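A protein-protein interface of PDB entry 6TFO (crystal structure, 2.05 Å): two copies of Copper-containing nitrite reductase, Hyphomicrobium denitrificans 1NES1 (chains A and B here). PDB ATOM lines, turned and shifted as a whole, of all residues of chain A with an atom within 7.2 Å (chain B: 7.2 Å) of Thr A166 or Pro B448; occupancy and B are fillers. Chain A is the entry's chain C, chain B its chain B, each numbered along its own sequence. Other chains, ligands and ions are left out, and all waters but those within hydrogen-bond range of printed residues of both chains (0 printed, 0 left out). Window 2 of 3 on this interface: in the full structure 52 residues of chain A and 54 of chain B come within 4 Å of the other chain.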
ATOM      1  N   ARG A 162     -12.013  33.245  -4.279  1.00  0.00           N
ATOM      2  CA  ARG A 162     -13.054  32.249  -4.636  1.00  0.00           C
ATOM      3  C   ARG A 162     -12.849  31.044  -3.724  1.00  0.00           C
ATOM      4  O   ARG A 162     -11.770  30.968  -3.075  1.00  0.00           O
ATOM      5  CB  ARG A 162     -13.010  31.836  -6.112  1.00  0.00           C
ATOM      6  CG  ARG A 162     -11.787  31.022  -6.523  1.00  0.00           C
ATOM      7  CD  ARG A 162     -12.006  30.044  -7.694  1.00  0.00           C
ATOM      8  NE  ARG A 162     -10.788  29.395  -8.224  1.00  0.00           N
ATOM      9  CZ  ARG A 162     -10.186  28.304  -7.710  1.00  0.00           C
ATOM     10  NH1 ARG A 162     -10.677  27.684  -6.645  1.00  0.00           N
ATOM     11  NH2 ARG A 162      -9.082  27.839  -8.262  1.00  0.00           N
ATOM     12  N   GLN A 163     -13.846  30.159  -3.652  1.00  0.00           N
ATOM     13  CA  GLN A 163     -13.754  28.928  -2.827  1.00  0.00           C
ATOM     14  C   GLN A 163     -12.863  27.916  -3.561  1.00  0.00           C
ATOM     15  O   GLN A 163     -12.832  27.952  -4.818  1.00  0.00           O
ATOM     16  CB  GLN A 163     -15.145  28.349  -2.535  1.00  0.00           C
ATOM     17  CG  GLN A 163     -15.522  28.302  -1.057  1.00  0.00           C
ATOM     18  CD  GLN A 163     -15.838  29.664  -0.495  1.00  0.00           C
ATOM     19  OE1 GLN A 163     -14.945  30.394  -0.064  1.00  0.00           O
ATOM     20  NE2 GLN A 163     -17.116  30.009  -0.507  1.00  0.00           N
ATOM     21  N   ALA A 164     -12.191  27.045  -2.800  1.00  0.00           N
ATOM     22  CA  ALA A 164     -11.584  25.796  -3.304  1.00  0.00           C
ATOM     23  C   ALA A 164     -12.602  25.123  -4.227  1.00  0.00           C
ATOM     24  O   ALA A 164     -13.815  25.271  -3.979  1.00  0.00           O
ATOM     25  CB  ALA A 164     -11.200  24.898  -2.153  1.00  0.00           C
ATOM     26  N   LYS A 165     -12.139  24.440  -5.273  1.00  0.00           N
ATOM     27  CA  LYS A 165     -13.022  23.724  -6.234  1.00  0.00           C
ATOM     28  C   LYS A 165     -12.214  22.655  -6.980  1.00  0.00           C
ATOM     29  O   LYS A 165     -10.977  22.585  -6.799  1.00  0.00           O
ATOM     30  CB  LYS A 165     -13.671  24.708  -7.214  1.00  0.00           C
ATOM     31  CG  LYS A 165     -12.706  25.338  -8.200  1.00  0.00           C
ATOM     32  CD  LYS A 165     -13.198  26.582  -8.876  1.00  0.00           C
ATOM     33  CE  LYS A 165     -12.541  26.778 -10.227  1.00  0.00           C
ATOM     34  NZ  LYS A 165     -13.424  27.484 -11.182  1.00  0.00           N
ATOM     35  N   THR A 166     -12.908  21.859  -7.789  1.00  0.00           N
ATOM     36  CA  THR A 166     -12.305  20.895  -8.736  1.00  0.00           C
ATOM     37  C   THR A 166     -11.866  21.660  -9.989  1.00  0.00           C
ATOM     38  O   THR A 166     -12.715  22.346 -10.575  1.00  0.00           O
ATOM     39  CB  THR A 166     -13.280  19.760  -9.047  1.00  0.00           C
ATOM     40  OG1 THR A 166     -13.361  18.962  -7.869  1.00  0.00           O
ATOM     41  CG2 THR A 166     -12.843  18.909 -10.220  1.00  0.00           C
ATOM     42  N   VAL A 167     -10.583  21.545 -10.356  1.00  0.00           N
ATOM     43  CA  VAL A 167      -9.947  22.181 -11.553  1.00  0.00           C
ATOM     44  C   VAL A 167      -9.431  21.071 -12.486  1.00  0.00           C
ATOM     45  O   VAL A 167      -8.567  20.279 -12.058  1.00  0.00           O
ATOM     46  CB  VAL A 167      -8.803  23.133 -11.141  1.00  0.00           C
ATOM     47  CG1 VAL A 167      -8.187  23.845 -12.333  1.00  0.00           C
ATOM     48  CG2 VAL A 167      -9.254  24.149 -10.126  1.00  0.00           C
ATOM     49  N   ARG A 168      -9.925  21.029 -13.722  1.00  0.00           N
ATOM     50  CA  ARG A 168      -9.444  20.090 -14.771  1.00  0.00           C
ATOM     51  C   ARG A 168      -8.264  20.746 -15.486  1.00  0.00           C
ATOM     52  O   ARG A 168      -8.420  21.881 -15.982  1.00  0.00           O
ATOM     53  CB  ARG A 168     -10.536  19.747 -15.787  1.00  0.00           C
ATOM     54  CG  ARG A 168     -10.172  18.607 -16.726  1.00  0.00           C
ATOM     55  CD  ARG A 168     -10.676  18.828 -18.136  1.00  0.00           C
ATOM     56  NE  ARG A 168     -10.148  17.825 -19.051  1.00  0.00           N
ATOM     57  CZ  ARG A 168     -10.809  16.764 -19.517  1.00  0.00           C
ATOM     58  NH1 ARG A 168     -12.058  16.523 -19.171  1.00  0.00           N
ATOM     59  NH2 ARG A 168     -10.203  15.935 -20.345  1.00  0.00           N
ATOM     60  N   GLY A 205      -6.235  23.843  -1.446  1.00  0.00           N
ATOM     61  CA  GLY A 205      -7.539  23.192  -1.211  1.00  0.00           C
ATOM     62  C   GLY A 205      -8.184  22.686  -2.489  1.00  0.00           C
ATOM     63  O   GLY A 205      -8.991  21.748  -2.383  1.00  0.00           O
ATOM     64  N   ASP A 206      -7.846  23.251  -3.653  1.00  0.00           N
ATOM     65  CA  ASP A 206      -8.377  22.792  -4.963  1.00  0.00           C
ATOM     66  C   ASP A 206      -8.129  21.286  -5.140  1.00  0.00           C
ATOM     67  O   ASP A 206      -7.128  20.766  -4.604  1.00  0.00           O
ATOM     68  CB  ASP A 206      -7.774  23.563  -6.134  1.00  0.00           C
ATOM     69  CG  ASP A 206      -8.384  24.934  -6.339  1.00  0.00           C
ATOM     70  OD1 ASP A 206      -9.395  25.196  -5.704  1.00  0.00           O
ATOM     71  OD2 ASP A 206      -7.834  25.721  -7.140  1.00  0.00           O
ATOM     72  N   THR A 207      -9.046  20.618  -5.841  1.00  0.00           N
ATOM     73  CA  THR A 207      -8.893  19.226  -6.337  1.00  0.00           C
ATOM     74  C   THR A 207      -8.544  19.307  -7.831  1.00  0.00           C
ATOM     75  O   THR A 207      -9.343  19.885  -8.600  1.00  0.00           O
ATOM     76  CB  THR A 207     -10.145  18.403  -5.992  1.00  0.00           C
ATOM     77  OG1 THR A 207     -10.057  18.112  -4.597  1.00  0.00           O
ATOM     78  CG2 THR A 207     -10.259  17.098  -6.751  1.00  0.00           C
ATOM     79  N   VAL A 208      -7.367  18.805  -8.212  1.00  0.00           N
ATOM     80  CA  VAL A 208      -6.833  18.868  -9.608  1.00  0.00           C
ATOM     81  C   VAL A 208      -7.161  17.540 -10.289  1.00  0.00           C
ATOM     82  O   VAL A 208      -6.762  16.467  -9.744  1.00  0.00           O
ATOM     83  CB  VAL A 208      -5.324  19.187  -9.641  1.00  0.00           C
ATOM     84  CG1 VAL A 208      -4.743  19.040 -11.035  1.00  0.00           C
ATOM     85  CG2 VAL A 208      -5.025  20.579  -9.084  1.00  0.00           C
ATOM     86  N   GLU A 209      -7.946  17.625 -11.369  1.00  0.00           N
ATOM     87  CA  GLU A 209      -8.290  16.512 -12.287  1.00  0.00           C
ATOM     88  C   GLU A 209      -7.366  16.641 -13.494  1.00  0.00           C
ATOM     89  O   GLU A 209      -7.671  17.447 -14.409  1.00  0.00           O
ATOM     90  CB  GLU A 209      -9.758  16.571 -12.708  1.00  0.00           C
ATOM     91  CG  GLU A 209     -10.166  15.510 -13.714  1.00  0.00           C
ATOM     92  CD  GLU A 209     -11.567  15.720 -14.263  1.00  0.00           C
ATOM     93  OE1 GLU A 209     -11.762  15.611 -15.483  1.00  0.00           O
ATOM     94  OE2 GLU A 209     -12.460  16.029 -13.461  1.00  0.00           O
ATOM     95  N   LEU A 210      -6.244  15.922 -13.455  1.00  0.00           N
ATOM     96  CA  LEU A 210      -5.187  16.026 -14.487  1.00  0.00           C
ATOM     97  C   LEU A 210      -5.397  14.961 -15.553  1.00  0.00           C
ATOM     98  O   LEU A 210      -5.391  13.764 -15.197  1.00  0.00           O
ATOM     99  CB  LEU A 210      -3.801  15.850 -13.884  1.00  0.00           C
ATOM    100  CG  LEU A 210      -2.717  16.070 -14.930  1.00  0.00           C
ATOM    101  CD1 LEU A 210      -2.245  17.517 -14.922  1.00  0.00           C
ATOM    102  CD2 LEU A 210      -1.582  15.098 -14.715  1.00  0.00           C
ATOM    103  N   HIS A 211      -5.537  15.410 -16.797  1.00  0.00           N
ATOM    104  CA  HIS A 211      -5.532  14.558 -18.010  1.00  0.00           C
ATOM    105  C   HIS A 211      -4.173  14.718 -18.701  1.00  0.00           C
ATOM    106  O   HIS A 211      -3.859  15.865 -19.102  1.00  0.00           O
ATOM    107  CB  HIS A 211      -6.698  14.957 -18.911  1.00  0.00           C
ATOM    108  CG  HIS A 211      -8.027  14.558 -18.369  1.00  0.00           C
ATOM    109  ND1 HIS A 211      -8.783  13.545 -18.938  1.00  0.00           N
ATOM    110  CD2 HIS A 211      -8.731  15.008 -17.310  1.00  0.00           C
ATOM    111  CE1 HIS A 211      -9.902  13.402 -18.258  1.00  0.00           C
ATOM    112  NE2 HIS A 211      -9.895  14.290 -17.256  1.00  0.00           N
ATOM    113  N   VAL A 248      -5.447   9.762 -16.537  1.00  0.00           N
ATOM    114  CA  VAL A 248      -6.170  10.778 -15.732  1.00  0.00           C
ATOM    115  C   VAL A 248      -5.807  10.497 -14.280  1.00  0.00           C
ATOM    116  O   VAL A 248      -5.939   9.327 -13.877  1.00  0.00           O
ATOM    117  CB  VAL A 248      -7.688  10.702 -15.966  1.00  0.00           C
ATOM    118  CG1 VAL A 248      -8.401  11.822 -15.232  1.00  0.00           C
ATOM    119  CG2 VAL A 248      -8.038  10.724 -17.445  1.00  0.00           C
ATOM    120  N   VAL A 249      -5.315  11.499 -13.549  1.00  0.00           N
ATOM    121  CA  VAL A 249      -5.089  11.393 -12.077  1.00  0.00           C
ATOM    122  C   VAL A 249      -5.828  12.565 -11.411  1.00  0.00           C
ATOM    123  O   VAL A 249      -5.886  13.647 -12.019  1.00  0.00           O
ATOM    124  CB  VAL A 249      -3.580  11.357 -11.754  1.00  0.00           C
ATOM    125  CG1 VAL A 249      -2.877  12.655 -12.141  1.00  0.00           C
ATOM    126  CG2 VAL A 249      -3.326  11.015 -10.296  1.00  0.00           C
ATOM    127  N   THR A 250      -6.391  12.372 -10.219  1.00  0.00           N
ATOM    128  CA  THR A 250      -6.897  13.480  -9.367  1.00  0.00           C
ATOM    129  C   THR A 250      -5.984  13.588  -8.149  1.00  0.00           C
ATOM    130  O   THR A 250      -5.571  12.529  -7.621  1.00  0.00           O
ATOM    131  CB  THR A 250      -8.373  13.296  -9.010  1.00  0.00           C
ATOM    132  OG1 THR A 250      -8.783  11.988  -9.401  1.00  0.00           O
ATOM    133  CG2 THR A 250      -9.247  14.292  -9.729  1.00  0.00           C
ATOM    134  N   HIS B 444      -5.486   9.576  -6.667  1.00  0.00           N
ATOM    135  CA  HIS B 444      -6.114   8.352  -7.244  1.00  0.00           C
ATOM    136  C   HIS B 444      -6.171   8.417  -8.776  1.00  0.00           C
ATOM    137  O   HIS B 444      -6.002   9.516  -9.320  1.00  0.00           O
ATOM    138  CB  HIS B 444      -7.506   8.085  -6.617  1.00  0.00           C
ATOM    139  CG  HIS B 444      -8.564   9.094  -6.958  1.00  0.00           C
ATOM    140  ND1 HIS B 444      -8.954  10.089  -6.071  1.00  0.00           N
ATOM    141  CD2 HIS B 444      -9.346   9.248  -8.054  1.00  0.00           C
ATOM    142  CE1 HIS B 444      -9.902  10.824  -6.621  1.00  0.00           C
ATOM    143  NE2 HIS B 444     -10.152  10.333  -7.844  1.00  0.00           N
ATOM    144  N   GLY B 446      -8.776   7.613 -11.475  1.00  0.00           N
ATOM    145  CA  GLY B 446      -9.797   8.218 -12.363  1.00  0.00           C
ATOM    146  C   GLY B 446      -9.934   9.723 -12.118  1.00  0.00           C
ATOM    147  O   GLY B 446      -9.137  10.319 -11.384  1.00  0.00           O
ATOM    148  N   PRO B 447     -10.996  10.376 -12.654  1.00  0.00           N
ATOM    149  CA  PRO B 447     -11.402  11.722 -12.212  1.00  0.00           C
ATOM    150  C   PRO B 447     -12.150  11.668 -10.867  1.00  0.00           C
ATOM    151  O   PRO B 447     -12.330  10.587 -10.315  1.00  0.00           O
ATOM    152  CB  PRO B 447     -12.260  12.207 -13.398  1.00  0.00           C
ATOM    153  CG  PRO B 447     -12.885  10.942 -13.953  1.00  0.00           C
ATOM    154  CD  PRO B 447     -11.885   9.833 -13.694  1.00  0.00           C
ATOM    155  N   PRO B 448     -12.598  12.795 -10.254  1.00  0.00           N
ATOM    156  CA  PRO B 448     -13.338  12.748  -8.989  1.00  0.00           C
ATOM    157  C   PRO B 448     -14.863  12.785  -9.167  1.00  0.00           C
ATOM    158  O   PRO B 448     -15.514  11.757  -9.084  1.00  0.00           O
ATOM    159  CB  PRO B 448     -12.878  14.050  -8.341  1.00  0.00           C
ATOM    160  CG  PRO B 448     -12.824  15.013  -9.524  1.00  0.00           C
ATOM    161  CD  PRO B 448     -12.455  14.177 -10.738  1.00  0.00           C
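The backbone carbonyl oxygen of Val A167 is in hydrogen-bond range of the backbone NH of Glu A209 (2.8 Å). The side-chain carboxylate (OE1) of Glu A209 lies within salt-bridge range of the guanidinium group (NH1) of Arg A168, 3.8 Å away. NE2 of His A211 sits at hydrogen-bond distance from OE1 of Glu A209, at 2.9 Å. O of Val A249 sits at hydrogen-bond distance from N of Leu A210 (2.7 Å). NE2 of His B444 sits at hydrogen-bond distance from O of Pro B447, 3.3 Å away.
Thr A166 touches one residue of chain B. Gly A205 touches none of the printed residues of chain B. Of the printed residues of chain B, Glu A209 touches Pro B447 and Pro B448. Printed residues of chain A within 4 Å of His B444: Val A249 and Thr A250. Of the printed residues of chain A, Pro B447 touches Glu A209 (3.7 Å), Val A248 (3.9 Å) and Thr A250 (3.7 Å). Pro B448 touches just these residues of chain A: Thr A166, Glu A209 and Thr A250. The nearest residue of chain A that does not touch Pro B448 is Thr A207 (4.3 Å).
No position is printed for both chains. Of the 10 pairs that touch across the chains among the printed residues, none has its exchanged pair printed and touching as well.
Along chain B the printed residues that touch a printed residue of chain A span positions 444 to 448. Of the 17 printed residues of chain A, 5 touch a printed residue of chain B. Along chain A the printed residues that touch a printed residue of chain B span positions 166 to 250. Among the printed residues, no Asp or Glu carboxylate lies within 4 Å of a Lys or Arg side-chain nitrogen of the other chain.
Among the printed residues, merely in contact across the chains: Val A249 with His B444 (3.2 Å), Glu A209 with Pro B448 (3.3 Å), Thr A250 with Pro B448 (3.4 Å), Glu A209 with Pro B447 (3.7 Å), Thr A250 with Pro B447 (3.7 Å), Val A248 with Pro B447 (3.9 Å), Thr A166 with Pro B448 (3.96 Å) and Val A249 with Gly B446 (3.999 Å).
NE2 of His B444 sits at hydrogen-bond distance from OG1 of Thr A250 (2.7 Å). O of Gly B446 sits at hydrogen-bond distance from OG1 of Thr A250, at 2.6 Å.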
